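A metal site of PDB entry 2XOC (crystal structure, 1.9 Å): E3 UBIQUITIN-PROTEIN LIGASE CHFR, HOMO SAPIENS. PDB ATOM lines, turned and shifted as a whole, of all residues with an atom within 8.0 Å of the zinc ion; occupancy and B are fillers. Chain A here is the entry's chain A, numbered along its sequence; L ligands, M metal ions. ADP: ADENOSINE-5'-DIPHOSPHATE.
The backbone NH (N) of Tyr 233 sits at hydrogen-bond distance from a nitrogen (N3) of the ligand, at 2.9 Å.
O3' of the ligand sits at hydrogen-bond distance from O of Asp 231, at 2.9 Å.
ND1 of His 252 lies within hydrogen-bond range of O of Phe 250.
The backbone NH (N) of Cys 232 sits at hydrogen-bond distance from the backbone carbonyl oxygen (O) of Asn 251, 3.0 Å away.
O of Cys 232 lies within hydrogen-bond range of SG of Cys 254 (3.8 Å).
The backbone NH (N) of Trp 234 lies close to the side-chain sulfur (SG) of Cys 232.
The backbone NH (N) of Thr 240 sits close to the side-chain sulfur (SG) of Cys 238.
The backbone carbonyl oxygen (O) of Cys 238 lies within hydrogen-bond range of the side-chain amide nitrogen (NE2) of Gln 241 (2.9 Å).
Four residues have an atom within 4 Å of the zinc ion: Cys 232, Cys 238, His 246 and His 252.
The nearest printed residue that does not touch the zinc ion is Trp 234 (4.5 Å).
The zinc ion is bound by a ring nitrogen (NE2) of His 246.
NE2 of His 252 binds the zinc ion.
The zinc ion is bound by SG of Cys 238, 2.3 Å away.
The side-chain sulfur (SG) of Cys 232 binds the zinc ion, at 2.3 Å.
The zinc ion has four donor atoms within binding distance.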
ATOM      1  N   ASN A 150      23.335   7.244  23.226  1.00  0.00           N
ATOM      2  CA  ASN A 150      22.266   8.062  23.762  1.00  0.00           C
ATOM      3  C   ASN A 150      21.016   7.202  23.939  1.00  0.00           C
ATOM      4  O   ASN A 150      20.375   6.827  22.951  1.00  0.00           O
ATOM      5  CB  ASN A 150      22.007   9.239  22.814  1.00  0.00           C
ATOM      6  CG  ASN A 150      20.931  10.180  23.321  1.00  0.00           C
ATOM      7  OD1 ASN A 150      19.954   9.761  23.954  1.00  0.00           O
ATOM      8  ND2 ASN A 150      21.081  11.458  23.022  1.00  0.00           N
ATOM      9  N   PRO A 230      13.761  20.749  19.764  1.00  0.00           N
ATOM     10  CA  PRO A 230      14.645  21.539  18.907  1.00  0.00           C
ATOM     11  C   PRO A 230      15.975  20.829  18.752  1.00  0.00           C
ATOM     12  O   PRO A 230      16.360  20.054  19.616  1.00  0.00           O
ATOM     13  CB  PRO A 230      14.861  22.835  19.710  1.00  0.00           C
ATOM     14  CG  PRO A 230      14.111  22.660  21.013  1.00  0.00           C
ATOM     15  CD  PRO A 230      13.798  21.209  21.162  1.00  0.00           C
ATOM     16  N   ASP A 231      16.667  21.107  17.648  1.00  0.00           N
ATOM     17  CA  ASP A 231      17.987  20.531  17.437  1.00  0.00           C
ATOM     18  C   ASP A 231      18.977  21.042  18.469  1.00  0.00           C
ATOM     19  O   ASP A 231      18.972  22.220  18.814  1.00  0.00           O
ATOM     20  CB  ASP A 231      18.497  20.901  16.037  1.00  0.00           C
ATOM     21  CG  ASP A 231      17.865  20.073  14.946  1.00  0.00           C
ATOM     22  OD1 ASP A 231      16.988  19.239  15.261  1.00  0.00           O
ATOM     23  OD2 ASP A 231      18.251  20.261  13.772  1.00  0.00           O
ATOM     24  N   CYS A 232      19.838  20.152  18.960  1.00  0.00           N
ATOM     25  CA  CYS A 232      20.961  20.611  19.772  1.00  0.00           C
ATOM     26  C   CYS A 232      22.005  21.262  18.867  1.00  0.00           C
ATOM     27  O   CYS A 232      22.351  20.738  17.811  1.00  0.00           O
ATOM     28  CB  CYS A 232      21.608  19.469  20.562  1.00  0.00           C
ATOM     29  SG  CYS A 232      23.085  20.025  21.460  1.00  0.00           S
ATOM     30  N   TYR A 233      22.493  22.417  19.305  1.00  0.00           N
ATOM     31  CA  TYR A 233      23.485  23.171  18.576  1.00  0.00           C
ATOM     32  C   TYR A 233      24.695  22.299  18.196  1.00  0.00           C
ATOM     33  O   TYR A 233      25.272  22.460  17.117  1.00  0.00           O
ATOM     34  CB  TYR A 233      23.935  24.364  19.429  1.00  0.00           C
ATOM     35  CG  TYR A 233      24.854  25.330  18.730  1.00  0.00           C
ATOM     36  CD1 TYR A 233      26.231  25.157  18.748  1.00  0.00           C
ATOM     37  CD2 TYR A 233      24.348  26.449  18.068  1.00  0.00           C
ATOM     38  CE1 TYR A 233      27.081  26.047  18.118  1.00  0.00           C
ATOM     39  CE2 TYR A 233      25.190  27.349  17.432  1.00  0.00           C
ATOM     40  CZ  TYR A 233      26.559  27.141  17.466  1.00  0.00           C
ATOM     41  OH  TYR A 233      27.399  28.032  16.834  1.00  0.00           O
ATOM     42  N   TRP A 234      25.046  21.371  19.073  1.00  0.00           N
ATOM     43  CA  TRP A 234      26.269  20.578  18.927  1.00  0.00           C
ATOM     44  C   TRP A 234      26.055  19.272  18.152  1.00  0.00           C
ATOM     45  O   TRP A 234      27.019  18.552  17.876  1.00  0.00           O
ATOM     46  CB  TRP A 234      26.881  20.288  20.296  1.00  0.00           C
ATOM     47  CG  TRP A 234      26.935  21.506  21.163  1.00  0.00           C
ATOM     48  CD1 TRP A 234      26.106  21.806  22.204  1.00  0.00           C
ATOM     49  CD2 TRP A 234      27.838  22.600  21.042  1.00  0.00           C
ATOM     50  NE1 TRP A 234      26.438  23.012  22.746  1.00  0.00           N
ATOM     51  CE2 TRP A 234      27.515  23.525  22.051  1.00  0.00           C
ATOM     52  CE3 TRP A 234      28.905  22.886  20.186  1.00  0.00           C
ATOM     53  CZ2 TRP A 234      28.209  24.714  22.228  1.00  0.00           C
ATOM     54  CZ3 TRP A 234      29.598  24.062  20.358  1.00  0.00           C
ATOM     55  CH2 TRP A 234      29.240  24.964  21.372  1.00  0.00           C
ATOM     56  N   GLY A 235      24.813  18.977  17.814  1.00  0.00           N
ATOM     57  CA  GLY A 235      24.502  17.834  16.974  1.00  0.00           C
ATOM     58  C   GLY A 235      24.866  16.483  17.541  1.00  0.00           C
ATOM     59  O   GLY A 235      24.992  16.326  18.763  1.00  0.00           O
ATOM     60  N   ARG A 236      25.067  15.510  16.658  1.00  0.00           N
ATOM     61  CA  ARG A 236      25.226  14.092  17.016  1.00  0.00           C
ATOM     62  C   ARG A 236      26.427  13.821  17.921  1.00  0.00           C
ATOM     63  O   ARG A 236      26.442  12.848  18.666  1.00  0.00           O
ATOM     64  CB  ARG A 236      25.333  13.240  15.749  1.00  0.00           C
ATOM     65  CG  ARG A 236      26.505  13.619  14.856  1.00  0.00           C
ATOM     66  CD  ARG A 236      26.409  12.976  13.470  1.00  0.00           C
ATOM     67  NE  ARG A 236      26.639  11.540  13.499  1.00  0.00           N
ATOM     68  CZ  ARG A 236      26.712  10.775  12.409  1.00  0.00           C
ATOM     69  NH1 ARG A 236      26.571  11.325  11.205  1.00  0.00           N
ATOM     70  NH2 ARG A 236      26.917   9.474  12.526  1.00  0.00           N
ATOM     71  N   ASN A 237      27.445  14.679  17.837  1.00  0.00           N
ATOM     72  CA  ASN A 237      28.653  14.479  18.629  1.00  0.00           C
ATOM     73  C   ASN A 237      28.617  15.175  19.987  1.00  0.00           C
ATOM     74  O   ASN A 237      29.606  15.184  20.724  1.00  0.00           O
ATOM     75  CB  ASN A 237      29.888  14.913  17.845  1.00  0.00           C
ATOM     76  CG  ASN A 237      30.127  14.047  16.621  1.00  0.00           C
ATOM     77  OD1 ASN A 237      30.012  12.823  16.684  1.00  0.00           O
ATOM     78  ND2 ASN A 237      30.446  14.674  15.488  1.00  0.00           N
ATOM     79  N   CYS A 238      27.476  15.761  20.318  1.00  0.00           N
ATOM     80  CA  CYS A 238      27.302  16.445  21.599  1.00  0.00           C
ATOM     81  C   CYS A 238      27.730  15.590  22.782  1.00  0.00           C
ATOM     82  O   CYS A 238      27.396  14.410  22.873  1.00  0.00           O
ATOM     83  CB  CYS A 238      25.856  16.884  21.786  1.00  0.00           C
ATOM     84  SG  CYS A 238      25.529  17.661  23.388  1.00  0.00           S
ATOM     85  N   ARG A 239      28.459  16.209  23.712  1.00  0.00           N
ATOM     86  CA  ARG A 239      29.033  15.500  24.850  1.00  0.00           C
ATOM     87  C   ARG A 239      28.050  15.435  26.020  1.00  0.00           C
ATOM     88  O   ARG A 239      28.230  14.665  26.956  1.00  0.00           O
ATOM     89  CB  ARG A 239      30.321  16.192  25.296  1.00  0.00           C
ATOM     90  CG  ARG A 239      31.324  16.369  24.187  1.00  0.00           C
ATOM     91  CD  ARG A 239      31.805  15.008  23.718  1.00  0.00           C
ATOM     92  NE  ARG A 239      33.125  14.673  24.247  1.00  0.00           N
ATOM     93  CZ  ARG A 239      34.190  14.433  23.493  1.00  0.00           C
ATOM     94  NH1 ARG A 239      35.361  14.151  24.058  1.00  0.00           N
ATOM     95  NH2 ARG A 239      34.087  14.496  22.175  1.00  0.00           N
ATOM     96  N   THR A 240      27.013  16.263  25.946  1.00  0.00           N
ATOM     97  CA  THR A 240      26.048  16.415  27.034  1.00  0.00           C
ATOM     98  C   THR A 240      24.893  15.433  26.939  1.00  0.00           C
ATOM     99  O   THR A 240      24.119  15.261  27.885  1.00  0.00           O
ATOM    100  CB  THR A 240      25.494  17.853  27.055  1.00  0.00           C
ATOM    101  OG1 THR A 240      26.556  18.794  26.881  1.00  0.00           O
ATOM    102  CG2 THR A 240      24.762  18.149  28.366  1.00  0.00           C
ATOM    103  N   GLN A 241      24.757  14.781  25.787  1.00  0.00           N
ATOM    104  CA  GLN A 241      23.599  13.904  25.549  1.00  0.00           C
ATOM    105  C   GLN A 241      23.629  12.607  26.355  1.00  0.00           C
ATOM    106  O   GLN A 241      22.652  11.855  26.372  1.00  0.00           O
ATOM    107  CB  GLN A 241      23.415  13.623  24.046  1.00  0.00           C
ATOM    108  CG  GLN A 241      24.534  12.826  23.408  1.00  0.00           C
ATOM    109  CD  GLN A 241      24.379  12.746  21.890  1.00  0.00           C
ATOM    110  OE1 GLN A 241      23.386  12.214  21.388  1.00  0.00           O
ATOM    111  NE2 GLN A 241      25.369  13.257  21.169  1.00  0.00           N
ATOM    112  N   VAL A 242      24.744  12.341  27.026  1.00  0.00           N
ATOM    113  CA  VAL A 242      24.792  11.192  27.921  1.00  0.00           C
ATOM    114  C   VAL A 242      24.035  11.509  29.216  1.00  0.00           C
ATOM    115  O   VAL A 242      23.822  10.633  30.051  1.00  0.00           O
ATOM    116  CB  VAL A 242      26.228  10.756  28.262  1.00  0.00           C
ATOM    117  CG1 VAL A 242      26.966  10.341  26.989  1.00  0.00           C
ATOM    118  CG2 VAL A 242      26.980  11.863  28.988  1.00  0.00           C
ATOM    119  N   HIS A 246      19.238  16.502  29.231  1.00  0.00           N
ATOM    120  CA  HIS A 246      19.637  17.142  27.994  1.00  0.00           C
ATOM    121  C   HIS A 246      19.211  16.311  26.785  1.00  0.00           C
ATOM    122  O   HIS A 246      18.793  16.857  25.768  1.00  0.00           O
ATOM    123  CB  HIS A 246      21.151  17.377  27.972  1.00  0.00           C
ATOM    124  CG  HIS A 246      21.620  18.107  26.750  1.00  0.00           C
ATOM    125  ND1 HIS A 246      21.522  19.476  26.619  1.00  0.00           N
ATOM    126  CD2 HIS A 246      22.195  17.657  25.610  1.00  0.00           C
ATOM    127  CE1 HIS A 246      22.014  19.840  25.446  1.00  0.00           C
ATOM    128  NE2 HIS A 246      22.428  18.759  24.814  1.00  0.00           N
ATOM    129  N   ALA A 247      19.327  14.994  26.916  1.00  0.00           N
ATOM    130  CA  ALA A 247      18.983  14.076  25.833  1.00  0.00           C
ATOM    131  C   ALA A 247      17.493  14.153  25.513  1.00  0.00           C
ATOM    132  O   ALA A 247      17.095  14.102  24.354  1.00  0.00           O
ATOM    133  CB  ALA A 247      19.378  12.635  26.191  1.00  0.00           C
ATOM    134  N   LYS A 249      15.544  16.782  26.151  1.00  0.00           N
ATOM    135  CA  LYS A 249      15.184  18.132  25.731  1.00  0.00           C
ATOM    136  C   LYS A 249      15.474  18.420  24.252  1.00  0.00           C
ATOM    137  O   LYS A 249      14.667  19.044  23.575  1.00  0.00           O
ATOM    138  CB  LYS A 249      15.882  19.171  26.629  1.00  0.00           C
ATOM    139  CG  LYS A 249      15.440  20.601  26.369  1.00  0.00           C
ATOM    140  CD  LYS A 249      16.016  21.545  27.414  1.00  0.00           C
ATOM    141  CE  LYS A 249      15.479  22.966  27.232  1.00  0.00           C
ATOM    142  NZ  LYS A 249      15.937  23.878  28.316  1.00  0.00           N
ATOM    143  N   PHE A 250      16.627  17.968  23.778  1.00  0.00           N
ATOM    144  CA  PHE A 250      17.077  18.281  22.418  1.00  0.00           C
ATOM    145  C   PHE A 250      17.170  17.065  21.509  1.00  0.00           C
ATOM    146  O   PHE A 250      17.528  15.972  21.948  1.00  0.00           O
ATOM    147  CB  PHE A 250      18.451  18.965  22.442  1.00  0.00           C
ATOM    148  CG  PHE A 250      18.466  20.289  23.148  1.00  0.00           C
ATOM    149  CD1 PHE A 250      18.821  20.365  24.490  1.00  0.00           C
ATOM    150  CD2 PHE A 250      18.157  21.457  22.477  1.00  0.00           C
ATOM    151  CE1 PHE A 250      18.859  21.589  25.137  1.00  0.00           C
ATOM    152  CE2 PHE A 250      18.185  22.682  23.121  1.00  0.00           C
ATOM    153  CZ  PHE A 250      18.537  22.736  24.462  1.00  0.00           C
ATOM    154  N   ASN A 251      16.868  17.273  20.229  1.00  0.00           N
ATOM    155  CA  ASN A 251      17.123  16.280  19.206  1.00  0.00           C
ATOM    156  C   ASN A 251      18.621  16.212  18.924  1.00  0.00           C
ATOM    157  O   ASN A 251      19.265  17.246  18.727  1.00  0.00           O
ATOM    158  CB  ASN A 251      16.370  16.606  17.918  1.00  0.00           C
ATOM    159  CG  ASN A 251      16.844  15.778  16.731  1.00  0.00           C
ATOM    160  OD1 ASN A 251      16.953  14.554  16.815  1.00  0.00           O
ATOM    161  ND2 ASN A 251      17.133  16.458  15.624  1.00  0.00           N
ATOM    162  N   HIS A 252      19.182  15.004  18.916  1.00  0.00           N
ATOM    163  CA  HIS A 252      20.594  14.839  18.597  1.00  0.00           C
ATOM    164  C   HIS A 252      20.820  14.059  17.306  1.00  0.00           C
ATOM    165  O   HIS A 252      21.937  13.660  17.002  1.00  0.00           O
ATOM    166  CB  HIS A 252      21.357  14.210  19.766  1.00  0.00           C
ATOM    167  CG  HIS A 252      21.547  15.134  20.930  1.00  0.00           C
ATOM    168  ND1 HIS A 252      20.624  15.247  21.955  1.00  0.00           N
ATOM    169  CD2 HIS A 252      22.539  16.012  21.204  1.00  0.00           C
ATOM    170  CE1 HIS A 252      21.054  16.145  22.814  1.00  0.00           C
ATOM    171  NE2 HIS A 252      22.204  16.625  22.387  1.00  0.00           N
ATOM    172  N   CYS A 254      21.133  15.179  14.288  1.00  0.00           N
ATOM    173  CA  CYS A 254      21.396  16.329  13.440  1.00  0.00           C
ATOM    174  C   CYS A 254      22.885  16.598  13.453  1.00  0.00           C
ATOM    175  O   CYS A 254      23.631  15.977  14.207  1.00  0.00           O
ATOM    176  CB  CYS A 254      20.618  17.554  13.942  1.00  0.00           C
ATOM    177  SG  CYS A 254      20.895  17.976  15.687  1.00  0.00           S
HETATM  178  PB  ADP L   1      18.141  30.533  16.409  1.00  0.00           P
HETATM  179  O1B ADP L   1      17.807  31.925  16.925  1.00  0.00           O
HETATM  180  O2B ADP L   1      18.036  30.455  14.900  1.00  0.00           O
HETATM  181  O3B ADP L   1      17.430  29.410  17.147  1.00  0.00           O
HETATM  182  PA  ADP L   1      20.377  29.675  18.050  1.00  0.00           P
HETATM  183  O1A ADP L   1      21.881  29.683  17.867  1.00  0.00           O
HETATM  184  O2A ADP L   1      19.779  30.263  19.310  1.00  0.00           O
HETATM  185  O3A ADP L   1      19.721  30.400  16.752  1.00  0.00           O
HETATM  186  O5' ADP L   1      19.910  28.129  17.980  1.00  0.00           O
HETATM  187  C5' ADP L   1      20.475  27.213  17.046  1.00  0.00           C
HETATM  188  C4' ADP L   1      20.141  25.814  17.551  1.00  0.00           C
HETATM  189  O4' ADP L   1      20.792  25.627  18.819  1.00  0.00           O
HETATM  190  C3' ADP L   1      18.641  25.677  17.776  1.00  0.00           C
HETATM  191  O3' ADP L   1      18.161  24.468  17.196  1.00  0.00           O
HETATM  192  C2' ADP L   1      18.463  25.573  19.276  1.00  0.00           C
HETATM  193  O2' ADP L   1      17.447  24.618  19.544  1.00  0.00           O
HETATM  194  C1' ADP L   1      19.831  25.087  19.742  1.00  0.00           C
HETATM  195  N9  ADP L   1      20.108  25.477  21.141  1.00  0.00           N
HETATM  196  C8  ADP L   1      19.670  26.554  21.826  1.00  0.00           C
HETATM  197  N7  ADP L   1      20.132  26.543  23.107  1.00  0.00           N
HETATM  198  C5  ADP L   1      20.883  25.427  23.259  1.00  0.00           C
HETATM  199  C6  ADP L   1      21.688  24.796  24.346  1.00  0.00           C
HETATM  200  N6  ADP L   1      21.779  25.350  25.583  1.00  0.00           N
HETATM  201  N1  ADP L   1      22.313  23.630  24.068  1.00  0.00           N
HETATM  202  C2  ADP L   1      22.237  23.055  22.844  1.00  0.00           C
HETATM  203  N3  ADP L   1      21.537  23.577  21.820  1.00  0.00           N
HETATM  204  C4  ADP L   1      20.850  24.732  21.967  1.00  0.00           C
HETATM  205 ZN    ZN M   1      23.338  18.312  23.013  1.00  0.00          ZN
